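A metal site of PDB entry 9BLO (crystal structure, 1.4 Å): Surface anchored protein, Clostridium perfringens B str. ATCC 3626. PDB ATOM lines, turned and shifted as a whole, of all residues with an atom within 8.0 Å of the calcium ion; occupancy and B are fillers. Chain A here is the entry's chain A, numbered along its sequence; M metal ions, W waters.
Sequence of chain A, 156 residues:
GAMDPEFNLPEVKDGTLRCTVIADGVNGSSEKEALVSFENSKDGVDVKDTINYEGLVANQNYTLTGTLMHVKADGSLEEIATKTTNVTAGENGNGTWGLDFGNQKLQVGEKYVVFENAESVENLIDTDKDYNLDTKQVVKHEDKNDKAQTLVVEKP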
ATOM      1  N   ALA A  23      -9.211  26.693  19.302  1.00  0.00           N
ATOM      2  CA  ALA A  23      -8.382  25.963  18.309  1.00  0.00           C
ATOM      3  C   ALA A  23      -8.753  26.475  16.924  1.00  0.00           C
ATOM      4  O   ALA A  23      -9.907  26.271  16.515  1.00  0.00           O
ATOM      5  CB  ALA A  23      -8.592  24.471  18.447  1.00  0.00           C
ATOM      6  N   ASP A  24      -7.833  27.188  16.259  1.00  0.00           N
ATOM      7  CA  ASP A  24      -8.098  27.895  14.986  1.00  0.00           C
ATOM      8  C   ASP A  24      -9.424  28.643  15.113  1.00  0.00           C
ATOM      9  O   ASP A  24     -10.264  28.527  14.204  1.00  0.00           O
ATOM     10  CB  ASP A  24      -8.080  26.931  13.801  1.00  0.00           C
ATOM     11  CG  ASP A  24      -6.703  26.766  13.191  1.00  0.00           C
ATOM     12  OD1 ASP A  24      -5.778  27.534  13.583  1.00  0.00           O
ATOM     13  OD2 ASP A  24      -6.575  25.875  12.333  1.00  0.00           O
ATOM     14  N   GLY A  25      -9.606  29.368  16.215  1.00  0.00           N
ATOM     15  CA  GLY A  25     -10.749  30.268  16.412  1.00  0.00           C
ATOM     16  C   GLY A  25     -11.997  29.568  16.936  1.00  0.00           C
ATOM     17  O   GLY A  25     -12.981  30.271  17.212  1.00  0.00           O
ATOM     18  N   VAL A  36     -11.865  21.444  14.668  1.00  0.00           N
ATOM     19  CA  VAL A  36     -11.030  22.215  13.704  1.00  0.00           C
ATOM     20  C   VAL A  36     -11.286  21.644  12.314  1.00  0.00           C
ATOM     21  O   VAL A  36     -11.085  20.441  12.137  1.00  0.00           O
ATOM     22  CB  VAL A  36      -9.538  22.162  14.070  1.00  0.00           C
ATOM     23  CG1 VAL A  36      -8.688  22.898  13.052  1.00  0.00           C
ATOM     24  CG2 VAL A  36      -9.280  22.685  15.480  1.00  0.00           C
ATOM     25  N   SER A  37     -11.708  22.476  11.363  1.00  0.00           N
ATOM     26  CA  SER A  37     -12.000  22.020   9.985  1.00  0.00           C
ATOM     27  C   SER A  37     -10.719  21.468   9.366  1.00  0.00           C
ATOM     28  O   SER A  37      -9.612  21.929   9.714  1.00  0.00           O
ATOM     29  CB  SER A  37     -12.595  23.113   9.148  1.00  0.00           C
ATOM     30  OG  SER A  37     -11.603  24.079   8.825  1.00  0.00           O
ATOM     31  N   PHE A  38     -10.869  20.511   8.465  1.00  0.00           N
ATOM     32  CA  PHE A  38      -9.734  19.961   7.699  1.00  0.00           C
ATOM     33  C   PHE A  38      -8.993  21.119   7.006  1.00  0.00           C
ATOM     34  O   PHE A  38      -7.765  21.169   7.063  1.00  0.00           O
ATOM     35  CB  PHE A  38     -10.218  18.912   6.701  1.00  0.00           C
ATOM     36  CG  PHE A  38      -9.161  18.586   5.679  1.00  0.00           C
ATOM     37  CD1 PHE A  38      -7.978  17.992   6.077  1.00  0.00           C
ATOM     38  CD2 PHE A  38      -9.322  18.926   4.354  1.00  0.00           C
ATOM     39  CE1 PHE A  38      -6.990  17.709   5.147  1.00  0.00           C
ATOM     40  CE2 PHE A  38      -8.334  18.643   3.423  1.00  0.00           C
ATOM     41  CZ  PHE A  38      -7.174  18.042   3.823  1.00  0.00           C
ATOM     42  N   GLU A  39      -9.717  22.022   6.342  1.00  0.00           N
ATOM     43  CA  GLU A  39      -9.079  23.142   5.598  1.00  0.00           C
ATOM     44  C   GLU A  39      -8.229  23.974   6.573  1.00  0.00           C
ATOM     45  O   GLU A  39      -7.087  24.308   6.205  1.00  0.00           O
ATOM     46  CB  GLU A  39     -10.135  24.009   4.908  1.00  0.00           C
ATOM     47  CG  GLU A  39      -9.553  25.050   3.969  1.00  0.00           C
ATOM     48  CD  GLU A  39      -8.731  24.515   2.804  1.00  0.00           C
ATOM     49  OE1 GLU A  39      -8.967  23.366   2.388  1.00  0.00           O
ATOM     50  OE2 GLU A  39      -7.841  25.248   2.336  1.00  0.00           O
ATOM     51  N   ASN A  40      -8.762  24.264   7.761  1.00  0.00           N
ATOM     52  CA  ASN A  40      -8.021  25.079   8.758  1.00  0.00           C
ATOM     53  C   ASN A  40      -6.809  24.306   9.258  1.00  0.00           C
ATOM     54  O   ASN A  40      -5.820  24.944   9.563  1.00  0.00           O
ATOM     55  CB  ASN A  40      -8.901  25.538   9.920  1.00  0.00           C
ATOM     56  CG  ASN A  40      -9.772  26.723   9.582  1.00  0.00           C
ATOM     57  OD1 ASN A  40      -9.645  27.313   8.510  1.00  0.00           O
ATOM     58  ND2 ASN A  40     -10.629  27.073  10.516  1.00  0.00           N
ATOM     59  N   SER A  41      -6.830  22.975   9.281  1.00  0.00           N
ATOM     60  CA  SER A  41      -5.675  22.172   9.772  1.00  0.00           C
ATOM     61  C   SER A  41      -4.464  22.290   8.846  1.00  0.00           C
ATOM     62  O   SER A  41      -3.359  21.987   9.304  1.00  0.00           O
ATOM     63  CB  SER A  41      -6.076  20.735   9.954  1.00  0.00           C
ATOM     64  OG  SER A  41      -6.018  20.026   8.719  1.00  0.00           O
ATOM     65  N   LYS A  42      -4.641  22.701   7.583  1.00  0.00           N
ATOM     66  CA  LYS A  42      -3.571  22.645   6.561  1.00  0.00           C
ATOM     67  C   LYS A  42      -2.379  23.542   6.910  1.00  0.00           C
ATOM     68  O   LYS A  42      -1.257  23.176   6.518  1.00  0.00           O
ATOM     69  CB  LYS A  42      -4.109  23.029   5.186  1.00  0.00           C
ATOM     70  CG  LYS A  42      -5.020  21.976   4.577  1.00  0.00           C
ATOM     71  CD  LYS A  42      -5.537  22.416   3.241  1.00  0.00           C
ATOM     72  CE  LYS A  42      -6.257  21.317   2.498  1.00  0.00           C
ATOM     73  NZ  LYS A  42      -6.795  21.800   1.219  1.00  0.00           N
ATOM     74  N   ASP A  43      -2.600  24.671   7.589  1.00  0.00           N
ATOM     75  CA  ASP A  43      -1.513  25.617   7.975  1.00  0.00           C
ATOM     76  C   ASP A  43      -1.225  25.440   9.470  1.00  0.00           C
ATOM     77  O   ASP A  43      -0.723  26.392  10.089  1.00  0.00           O
ATOM     78  CB  ASP A  43      -1.865  27.049   7.590  1.00  0.00           C
ATOM     79  CG  ASP A  43      -3.064  27.594   8.336  1.00  0.00           C
ATOM     80  OD1 ASP A  43      -3.713  26.800   9.023  1.00  0.00           O
ATOM     81  OD2 ASP A  43      -3.324  28.817   8.231  1.00  0.00           O
ATOM     82  N   GLY A  44      -1.506  24.259  10.020  1.00  0.00           N
ATOM     83  CA  GLY A  44      -1.367  23.994  11.458  1.00  0.00           C
ATOM     84  C   GLY A  44      -2.577  24.495  12.222  1.00  0.00           C
ATOM     85  O   GLY A  44      -3.521  24.962  11.582  1.00  0.00           O
ATOM     86  N   VAL A  45      -2.564  24.388  13.542  1.00  0.00           N
ATOM     87  CA  VAL A  45      -3.711  24.768  14.404  1.00  0.00           C
ATOM     88  C   VAL A  45      -3.189  25.728  15.467  1.00  0.00           C
ATOM     89  O   VAL A  45      -2.317  25.324  16.246  1.00  0.00           O
ATOM     90  CB  VAL A  45      -4.413  23.545  15.033  1.00  0.00           C
ATOM     91  CG1 VAL A  45      -5.608  23.964  15.870  1.00  0.00           C
ATOM     92  CG2 VAL A  45      -4.825  22.526  13.976  1.00  0.00           C
ATOM     93  N   ASP A  46      -3.713  26.948  15.470  1.00  0.00           N
ATOM     94  CA  ASP A  46      -3.409  27.944  16.532  1.00  0.00           C
ATOM     95  C   ASP A  46      -4.196  27.552  17.777  1.00  0.00           C
ATOM     96  O   ASP A  46      -5.430  27.539  17.716  1.00  0.00           O
ATOM     97  CB  ASP A  46      -3.737  29.354  16.043  1.00  0.00           C
ATOM     98  CG  ASP A  46      -2.978  29.740  14.787  1.00  0.00           C
ATOM     99  OD1 ASP A  46      -1.758  29.473  14.734  1.00  0.00           O
ATOM    100  OD2 ASP A  46      -3.620  30.271  13.859  1.00  0.00           O
ATOM    101  N   ASN A 103       1.149  28.141  16.884  1.00  0.00           N
ATOM    102  CA  ASN A 103       0.746  27.282  15.747  1.00  0.00           C
ATOM    103  C   ASN A 103       1.303  25.882  15.966  1.00  0.00           C
ATOM    104  O   ASN A 103       2.537  25.740  16.005  1.00  0.00           O
ATOM    105  CB  ASN A 103       1.203  27.890  14.426  1.00  0.00           C
ATOM    106  CG  ASN A 103       0.653  27.131  13.239  1.00  0.00           C
ATOM    107  OD1 ASN A 103       1.307  26.212  12.744  1.00  0.00           O
ATOM    108  ND2 ASN A 103      -0.547  27.462  12.821  1.00  0.00           N
ATOM    109  N   GLN A 104       0.430  24.889  16.125  1.00  0.00           N
ATOM    110  CA  GLN A 104       0.810  23.475  16.385  1.00  0.00           C
ATOM    111  C   GLN A 104       0.513  22.636  15.144  1.00  0.00           C
ATOM    112  O   GLN A 104      -0.567  22.804  14.562  1.00  0.00           O
ATOM    113  CB  GLN A 104       0.063  22.986  17.617  1.00  0.00           C
ATOM    114  CG  GLN A 104       0.467  23.726  18.885  1.00  0.00           C
ATOM    115  CD  GLN A 104       1.868  23.394  19.321  1.00  0.00           C
ATOM    116  OE1 GLN A 104       2.350  22.277  19.140  1.00  0.00           O
ATOM    117  NE2 GLN A 104       2.536  24.368  19.926  1.00  0.00           N
ATOM    118  N   LYS A 105       1.442  21.768  14.754  1.00  0.00           N
ATOM    119  CA  LYS A 105       1.279  20.902  13.557  1.00  0.00           C
ATOM    120  C   LYS A 105       0.542  19.638  14.006  1.00  0.00           C
ATOM    121  O   LYS A 105       1.179  18.580  14.216  1.00  0.00           O
ATOM    122  CB  LYS A 105       2.634  20.662  12.883  1.00  0.00           C
ATOM    123  CG  LYS A 105       3.334  21.926  12.388  1.00  0.00           C
ATOM    124  CD  LYS A 105       2.440  22.892  11.621  1.00  0.00           C
ATOM    125  CE  LYS A 105       3.189  24.123  11.142  1.00  0.00           C
ATOM    126  NZ  LYS A 105       2.306  25.032  10.368  1.00  0.00           N
HETATM  127 CA    CA M   1      -4.974  26.573  10.891  1.00  0.00          CA
HETATM  128  O   HOH W   1      -3.600  28.175  11.779  1.00  0.00           O
HETATM  129  O   HOH W   2      -6.410  28.104   9.952  1.00  0.00           O
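The side-chain hydroxyl of Ser 37 is in hydrogen-bond range of the backbone NH of Asn 40, at 3.0 Å. N of Asp 24 is in hydrogen-bond range of O of Asp 46 (2.8 Å). The side-chain amide nitrogen (ND2) of Asn 103 sits at hydrogen-bond distance from the backbone carbonyl oxygen (O) of Asp 43 (2.9 Å). The backbone carbonyl oxygen (O) of Asp 43 is in hydrogen-bond range of the side-chain amino group (NZ) of Lys 105, 3.3 Å away.
Four residues have an atom within 4 Å of the calcium ion: Asp 24, Asn 40, Asp 43 and Gly 44.
The side-chain carboxylate (OD2) of Asp 24 binds the calcium ion, 2.3 Å away. OD1 of Asp 43 binds the calcium ion. O of Asn 40 is bound to the calcium ion, at 2.3 Å. O of Gly 44 is bound to the calcium ion. The calcium ion is bound by water W1, 2.3 Å away. The calcium ion is bound by water W2. The calcium ion has six donor atoms within binding distance. Slightly farther from the calcium ion lies OD1 of Asp 24 (3.0 Å).
Water W1 lies within hydrogen-bond range of the side-chain carboxylate (OD1) of Asp 24 (2.9 Å), the side-chain carboxylate (OD2) of Asp 46 (3.0 Å) and the side-chain amide nitrogen (ND2) of Asn 103 (3.3 Å).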
